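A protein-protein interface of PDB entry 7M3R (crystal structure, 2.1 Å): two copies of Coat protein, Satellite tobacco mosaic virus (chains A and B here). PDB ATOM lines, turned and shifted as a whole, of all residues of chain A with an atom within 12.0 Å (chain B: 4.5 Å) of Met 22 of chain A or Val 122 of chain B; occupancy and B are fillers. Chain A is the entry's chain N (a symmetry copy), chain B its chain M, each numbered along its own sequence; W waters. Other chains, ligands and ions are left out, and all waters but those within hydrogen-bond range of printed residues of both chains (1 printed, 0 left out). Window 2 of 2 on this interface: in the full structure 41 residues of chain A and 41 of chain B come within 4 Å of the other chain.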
ATOM      1  N   SER A  17      27.095 -33.320   8.073  1.00  0.00           N
ATOM      2  CA  SER A  17      28.398 -33.414   8.715  1.00  0.00           C
ATOM      3  C   SER A  17      28.610 -34.814   9.276  1.00  0.00           C
ATOM      4  O   SER A  17      27.654 -35.525   9.600  1.00  0.00           O
ATOM      5  CB  SER A  17      28.532 -32.377   9.835  1.00  0.00           C
ATOM      6  OG  SER A  17      29.777 -32.500  10.500  1.00  0.00           O
ATOM      7  N   ASN A  18      29.881 -35.198   9.401  1.00  0.00           N
ATOM      8  CA  ASN A  18      30.252 -36.549   9.801  1.00  0.00           C
ATOM      9  C   ASN A  18      30.665 -36.666  11.262  1.00  0.00           C
ATOM     10  O   ASN A  18      31.020 -37.764  11.701  1.00  0.00           O
ATOM     11  CB  ASN A  18      31.400 -37.062   8.920  1.00  0.00           C
ATOM     12  CG  ASN A  18      30.984 -37.282   7.480  1.00  0.00           C
ATOM     13  OD1 ASN A  18      31.251 -36.455   6.613  1.00  0.00           O
ATOM     14  ND2 ASN A  18      30.332 -38.407   7.219  1.00  0.00           N
ATOM     15  N   VAL A  19      30.640 -35.575  12.028  1.00  0.00           N
ATOM     16  CA  VAL A  19      31.052 -35.601  13.426  1.00  0.00           C
ATOM     17  C   VAL A  19      30.145 -34.692  14.241  1.00  0.00           C
ATOM     18  O   VAL A  19      29.417 -33.854  13.704  1.00  0.00           O
ATOM     19  CB  VAL A  19      32.527 -35.177  13.608  1.00  0.00           C
ATOM     20  CG1 VAL A  19      33.462 -36.253  13.068  1.00  0.00           C
ATOM     21  CG2 VAL A  19      32.784 -33.845  12.922  1.00  0.00           C
ATOM     22  N   VAL A  20      30.201 -34.870  15.562  1.00  0.00           N
ATOM     23  CA  VAL A  20      29.372 -34.071  16.452  1.00  0.00           C
ATOM     24  C   VAL A  20      29.742 -32.596  16.320  1.00  0.00           C
ATOM     25  O   VAL A  20      30.903 -32.237  16.078  1.00  0.00           O
ATOM     26  CB  VAL A  20      29.520 -34.543  17.909  1.00  0.00           C
ATOM     27  CG1 VAL A  20      28.922 -35.931  18.083  1.00  0.00           C
ATOM     28  CG2 VAL A  20      30.986 -34.529  18.330  1.00  0.00           C
ATOM     29  N   THR A  21      28.739 -31.735  16.475  1.00  0.00           N
ATOM     30  CA  THR A  21      28.922 -30.292  16.448  1.00  0.00           C
ATOM     31  C   THR A  21      28.297 -29.692  17.698  1.00  0.00           C
ATOM     32  O   THR A  21      27.437 -30.299  18.339  1.00  0.00           O
ATOM     33  CB  THR A  21      28.302 -29.663  15.194  1.00  0.00           C
ATOM     34  OG1 THR A  21      26.923 -30.041  15.096  1.00  0.00           O
ATOM     35  CG2 THR A  21      29.047 -30.121  13.946  1.00  0.00           C
ATOM     36  N   MET A  22      28.738 -28.486  18.039  1.00  0.00           N
ATOM     37  CA  MET A  22      28.280 -27.818  19.248  1.00  0.00           C
ATOM     38  C   MET A  22      27.006 -27.030  18.975  1.00  0.00           C
ATOM     39  O   MET A  22      26.832 -26.446  17.902  1.00  0.00           O
ATOM     40  CB  MET A  22      29.364 -26.884  19.791  1.00  0.00           C
ATOM     41  CG  MET A  22      28.967 -26.155  21.068  1.00  0.00           C
ATOM     42  SD  MET A  22      30.330 -25.972  22.237  1.00  0.00           S
ATOM     43  CE  MET A  22      31.478 -24.980  21.283  1.00  0.00           C
ATOM     44  N   ILE A  23      26.113 -27.027  19.960  1.00  0.00           N
ATOM     45  CA  ILE A  23      24.876 -26.260  19.919  1.00  0.00           C
ATOM     46  C   ILE A  23      25.015 -25.131  20.931  1.00  0.00           C
ATOM     47  O   ILE A  23      25.298 -25.376  22.111  1.00  0.00           O
ATOM     48  CB  ILE A  23      23.652 -27.132  20.232  1.00  0.00           C
ATOM     49  CG1 ILE A  23      23.560 -28.299  19.248  1.00  0.00           C
ATOM     50  CG2 ILE A  23      22.381 -26.292  20.178  1.00  0.00           C
ATOM     51  CD1 ILE A  23      22.547 -29.356  19.643  1.00  0.00           C
ATOM     52  N   ARG A  24      24.831 -23.893  20.470  1.00  0.00           N
ATOM     53  CA  ARG A  24      24.910 -22.719  21.339  1.00  0.00           C
ATOM     54  C   ARG A  24      23.556 -22.509  22.018  1.00  0.00           C
ATOM     55  O   ARG A  24      22.799 -21.582  21.719  1.00  0.00           O
ATOM     56  CB  ARG A  24      25.342 -21.498  20.541  1.00  0.00           C
ATOM     57  CG  ARG A  24      26.779 -21.564  20.059  1.00  0.00           C
ATOM     58  CD  ARG A  24      27.103 -20.436  19.097  1.00  0.00           C
ATOM     59  NE  ARG A  24      28.530 -20.382  18.801  1.00  0.00           N
ATOM     60  CZ  ARG A  24      29.161 -21.232  18.001  1.00  0.00           C
ATOM     61  NH1 ARG A  24      28.522 -22.228  17.409  1.00  0.00           N
ATOM     62  NH2 ARG A  24      30.465 -21.079  17.791  1.00  0.00           N
ATOM     63  N   ALA A  25      23.257 -23.407  22.952  1.00  0.00           N
ATOM     64  CA  ALA A  25      21.999 -23.346  23.677  1.00  0.00           C
ATOM     65  C   ALA A  25      21.890 -22.034  24.448  1.00  0.00           C
ATOM     66  O   ALA A  25      22.873 -21.318  24.663  1.00  0.00           O
ATOM     67  CB  ALA A  25      21.874 -24.532  24.634  1.00  0.00           C
ATOM     68  N   GLY A  26      20.666 -21.723  24.869  1.00  0.00           N
ATOM     69  CA  GLY A  26      20.405 -20.499  25.599  1.00  0.00           C
ATOM     70  C   GLY A  26      19.666 -20.734  26.899  1.00  0.00           C
ATOM     71  O   GLY A  26      20.102 -21.533  27.732  1.00  0.00           O
ATOM     72  N   SER A  27      18.544 -20.044  27.085  1.00  0.00           N
ATOM     73  CA  SER A  27      17.759 -20.186  28.300  1.00  0.00           C
ATOM     74  C   SER A  27      16.965 -21.487  28.273  1.00  0.00           C
ATOM     75  O   SER A  27      16.523 -21.946  27.216  1.00  0.00           O
ATOM     76  CB  SER A  27      16.810 -19.000  28.464  1.00  0.00           C
ATOM     77  OG  SER A  27      17.514 -17.775  28.383  1.00  0.00           O
ATOM     78  N   TYR A  28      16.790 -22.079  29.448  1.00  0.00           N
ATOM     79  CA  TYR A  28      16.037 -23.319  29.552  1.00  0.00           C
ATOM     80  C   TYR A  28      14.662 -23.130  28.910  1.00  0.00           C
ATOM     81  O   TYR A  28      13.963 -22.159  29.232  1.00  0.00           O
ATOM     82  CB  TYR A  28      15.889 -23.736  31.015  1.00  0.00           C
ATOM     83  CG  TYR A  28      15.408 -25.160  31.195  1.00  0.00           C
ATOM     84  CD1 TYR A  28      16.308 -26.214  31.246  1.00  0.00           C
ATOM     85  CD2 TYR A  28      14.054 -25.448  31.305  1.00  0.00           C
ATOM     86  CE1 TYR A  28      15.874 -27.518  31.407  1.00  0.00           C
ATOM     87  CE2 TYR A  28      13.609 -26.749  31.463  1.00  0.00           C
ATOM     88  CZ  TYR A  28      14.524 -27.778  31.514  1.00  0.00           C
ATOM     89  OH  TYR A  28      14.087 -29.075  31.673  1.00  0.00           O
ATOM     90  N   PRO A  29      14.246 -24.009  28.008  1.00  0.00           N
ATOM     91  CA  PRO A  29      12.991 -23.796  27.281  1.00  0.00           C
ATOM     92  C   PRO A  29      11.792 -24.238  28.114  1.00  0.00           C
ATOM     93  O   PRO A  29      11.921 -24.772  29.213  1.00  0.00           O
ATOM     94  CB  PRO A  29      13.166 -24.667  26.035  1.00  0.00           C
ATOM     95  CG  PRO A  29      13.983 -25.829  26.530  1.00  0.00           C
ATOM     96  CD  PRO A  29      14.915 -25.258  27.588  1.00  0.00           C
ATOM     97  N   VAL B  78      21.766 -33.343  22.284  1.00  0.00           N
ATOM     98  CA  VAL B  78      21.753 -33.256  23.739  1.00  0.00           C
ATOM     99  C   VAL B  78      21.987 -31.807  24.145  1.00  0.00           C
ATOM    100  O   VAL B  78      22.879 -31.142  23.608  1.00  0.00           O
ATOM    101  CB  VAL B  78      22.820 -34.168  24.376  1.00  0.00           C
ATOM    102  CG1 VAL B  78      22.888 -33.930  25.884  1.00  0.00           C
ATOM    103  CG2 VAL B  78      22.524 -35.630  24.072  1.00  0.00           C
ATOM    104  N   ARG B  79      21.191 -31.324  25.094  1.00  0.00           N
ATOM    105  CA  ARG B  79      21.329 -29.978  25.632  1.00  0.00           C
ATOM    106  C   ARG B  79      21.256 -30.054  27.149  1.00  0.00           C
ATOM    107  O   ARG B  79      20.373 -30.722  27.696  1.00  0.00           O
ATOM    108  CB  ARG B  79      20.240 -29.049  25.086  1.00  0.00           C
ATOM    109  CG  ARG B  79      20.353 -28.767  23.594  1.00  0.00           C
ATOM    110  CD  ARG B  79      19.152 -27.974  23.097  1.00  0.00           C
ATOM    111  NE  ARG B  79      19.285 -27.567  21.703  1.00  0.00           N
ATOM    112  CZ  ARG B  79      18.887 -28.293  20.666  1.00  0.00           C
ATOM    113  NH1 ARG B  79      18.352 -29.491  20.826  1.00  0.00           N
ATOM    114  NH2 ARG B  79      19.031 -27.805  19.438  1.00  0.00           N
ATOM    115  N   ALA B  80      22.184 -29.377  27.823  1.00  0.00           N
ATOM    116  CA  ALA B  80      22.284 -29.417  29.272  1.00  0.00           C
ATOM    117  C   ALA B  80      22.248 -28.012  29.854  1.00  0.00           C
ATOM    118  O   ALA B  80      22.725 -27.052  29.241  1.00  0.00           O
ATOM    119  CB  ALA B  80      23.574 -30.123  29.721  1.00  0.00           C
ATOM    120  N   VAL B  94      29.175 -26.022  32.538  1.00  0.00           N
ATOM    121  CA  VAL B  94      28.798 -27.408  32.286  1.00  0.00           C
ATOM    122  C   VAL B  94      29.563 -27.887  31.063  1.00  0.00           C
ATOM    123  O   VAL B  94      29.766 -27.133  30.106  1.00  0.00           O
ATOM    124  CB  VAL B  94      27.273 -27.557  32.088  1.00  0.00           C
ATOM    125  CG1 VAL B  94      26.817 -26.813  30.841  1.00  0.00           C
ATOM    126  CG2 VAL B  94      26.890 -29.033  32.009  1.00  0.00           C
ATOM    127  N   LEU B  96      30.029 -31.365  28.318  1.00  0.00           N
ATOM    128  CA  LEU B  96      29.458 -32.598  27.794  1.00  0.00           C
ATOM    129  C   LEU B  96      30.504 -33.308  26.951  1.00  0.00           C
ATOM    130  O   LEU B  96      31.103 -32.698  26.060  1.00  0.00           O
ATOM    131  CB  LEU B  96      28.208 -32.321  26.948  1.00  0.00           C
ATOM    132  CG  LEU B  96      27.018 -31.655  27.634  1.00  0.00           C
ATOM    133  CD1 LEU B  96      25.963 -31.271  26.606  1.00  0.00           C
ATOM    134  CD2 LEU B  96      26.429 -32.568  28.692  1.00  0.00           C
ATOM    135  N   PHE B 109      32.477 -30.162  25.013  1.00  0.00           N
ATOM    136  CA  PHE B 109      31.660 -28.985  24.740  1.00  0.00           C
ATOM    137  C   PHE B 109      31.272 -28.312  26.049  1.00  0.00           C
ATOM    138  O   PHE B 109      30.594 -28.914  26.887  1.00  0.00           O
ATOM    139  CB  PHE B 109      30.416 -29.383  23.949  1.00  0.00           C
ATOM    140  CG  PHE B 109      30.719 -30.141  22.690  1.00  0.00           C
ATOM    141  CD1 PHE B 109      31.175 -29.483  21.564  1.00  0.00           C
ATOM    142  CD2 PHE B 109      30.547 -31.514  22.634  1.00  0.00           C
ATOM    143  CE1 PHE B 109      31.454 -30.178  20.402  1.00  0.00           C
ATOM    144  CE2 PHE B 109      30.827 -32.216  21.477  1.00  0.00           C
ATOM    145  CZ  PHE B 109      31.282 -31.547  20.360  1.00  0.00           C
ATOM    146  N   GLU B 110      31.702 -27.066  26.228  1.00  0.00           N
ATOM    147  CA  GLU B 110      31.547 -26.372  27.498  1.00  0.00           C
ATOM    148  C   GLU B 110      30.856 -25.033  27.304  1.00  0.00           C
ATOM    149  O   GLU B 110      31.154 -24.293  26.362  1.00  0.00           O
ATOM    150  CB  GLU B 110      32.909 -26.152  28.178  1.00  0.00           C
ATOM    151  CG  GLU B 110      32.833 -25.358  29.477  1.00  0.00           C
ATOM    152  CD  GLU B 110      34.173 -25.249  30.182  1.00  0.00           C
ATOM    153  OE1 GLU B 110      35.220 -25.384  29.511  1.00  0.00           O
ATOM    154  OE2 GLU B 110      34.180 -25.031  31.411  1.00  0.00           O
ATOM    155  N   GLY B 111      29.939 -24.735  28.206  1.00  0.00           N
ATOM    156  CA  GLY B 111      29.325 -23.419  28.266  1.00  0.00           C
ATOM    157  C   GLY B 111      29.406 -22.873  29.673  1.00  0.00           C
ATOM    158  O   GLY B 111      29.241 -23.608  30.645  1.00  0.00           O
ATOM    159  N   SER B 121      24.838 -23.199  29.957  1.00  0.00           N
ATOM    160  CA  SER B 121      24.215 -24.106  29.007  1.00  0.00           C
ATOM    161  C   SER B 121      25.167 -24.431  27.867  1.00  0.00           C
ATOM    162  O   SER B 121      26.034 -23.631  27.510  1.00  0.00           O
ATOM    163  CB  SER B 121      22.922 -23.503  28.430  1.00  0.00           C
ATOM    164  OG  SER B 121      23.208 -22.383  27.609  1.00  0.00           O
ATOM    165  N   VAL B 122      24.989 -25.622  27.297  1.00  0.00           N
ATOM    166  CA  VAL B 122      25.713 -26.028  26.099  1.00  0.00           C
ATOM    167  C   VAL B 122      25.036 -27.279  25.562  1.00  0.00           C
ATOM    168  O   VAL B 122      24.241 -27.913  26.262  1.00  0.00           O
ATOM    169  CB  VAL B 122      27.213 -26.267  26.419  1.00  0.00           C
ATOM    170  CG1 VAL B 122      27.411 -27.591  27.137  1.00  0.00           C
ATOM    171  CG2 VAL B 122      28.049 -26.203  25.147  1.00  0.00           C
ATOM    172  N   GLY B 123      25.336 -27.627  24.314  1.00  0.00           N
ATOM    173  CA  GLY B 123      24.777 -28.822  23.711  1.00  0.00           C
ATOM    174  C   GLY B 123      25.608 -29.248  22.521  1.00  0.00           C
ATOM    175  O   GLY B 123      26.492 -28.524  22.060  1.00  0.00           O
ATOM    176  N   TYR B 124      25.314 -30.447  22.026  1.00  0.00           N
ATOM    177  CA  TYR B 124      26.010 -30.972  20.860  1.00  0.00           C
ATOM    178  C   TYR B 124      25.053 -31.825  20.041  1.00  0.00           C
ATOM    179  O   TYR B 124      24.230 -32.561  20.596  1.00  0.00           O
ATOM    180  CB  TYR B 124      27.249 -31.789  21.261  1.00  0.00           C
ATOM    181  CG  TYR B 124      26.951 -33.118  21.925  1.00  0.00           C
ATOM    182  CD1 TYR B 124      26.762 -34.270  21.169  1.00  0.00           C
ATOM    183  CD2 TYR B 124      26.870 -33.223  23.308  1.00  0.00           C
ATOM    184  CE1 TYR B 124      26.490 -35.482  21.769  1.00  0.00           C
ATOM    185  CE2 TYR B 124      26.598 -34.433  23.917  1.00  0.00           C
ATOM    186  CZ  TYR B 124      26.413 -35.560  23.143  1.00  0.00           C
ATOM    187  OH  TYR B 124      26.144 -36.768  23.745  1.00  0.00           O
HETATM  188  O   HOH W   1      21.587 -20.707  29.916  1.00  0.00           O
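No position is printed for both chains.
Among the printed residues, merely in contact across the chains: Val 20 of chain A with Phe 109 of chain B, Thr 21 of chain A with Tyr 124 of chain B, Met 22 of chain A with Phe 109 of chain B, Met 22 of chain A with Val 122 of chain B, Met 22 of chain A with Gly 123 of chain B, Ile 23 of chain A with Arg 79 of chain B, Ile 23 of chain A with Val 122 of chain B and Ile 23 of chain A with Tyr 124 of chain B.
The backbone carbonyl oxygen (O) of Val 78 of chain B is in hydrogen-bond range of the backbone NH (N) of Tyr 124 of chain B (3.0 Å). The backbone NH of Ala 80 of chain B sits at hydrogen-bond distance from the backbone carbonyl oxygen of Val 122 of chain B (3.0 Å). N of Leu 96 of chain B is in hydrogen-bond range of O of Phe 109 of chain B, 2.9 Å away.
Water W1 lies within hydrogen-bond range of O of Gly 26 of chain A and OG of Ser 121 of chain B.
The side-chain hydroxyl (OG) of Ser 121 of chain B lies within hydrogen-bond range of the backbone carbonyl oxygen (O) of Ala 25 of chain A. OG of Ser 121 of chain B sits at hydrogen-bond distance from O of Gly 26 of chain A (3.2 Å). N of Ile 23 of chain A is in hydrogen-bond range of O of Gly 123 of chain B.
Of the 13 printed residues of chain A, 6 touch a printed residue of chain B. Among the printed residues, 11 pairs touch across the chains.
Of the printed residues of chain B, Met 22 of chain A touches Phe 109, Val 122 and Gly 123. Of the printed residues of chain A, Val 122 of chain B touches Met 22 (3.7 Å) and Ile 23 (3.9 Å). No residue of chain A comes within 4 Å of Ala 80 of chain B. No residue of chain A comes within 4 Å of Gly 111 of chain B. Of the printed residues of chain A, Phe 109 of chain B touches Val 20 (3.6 Å) and Met 22 (3.6 Å). Printed residues of chain B within 4 Å of Ile 23 of chain A: Arg 79 (3.7 Å), Val 122 (3.9 Å), Gly 123 (2.6 Å) and Tyr 124 (3.5 Å). Printed residues of chain A within 4 Å of Tyr 124 of chain B: Thr 21 (3.0 Å) and Ile 23 (3.5 Å). The nearest printed residue of chain B that does not touch Met 22 of chain A is Tyr 124 of chain B (4.2 Å).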
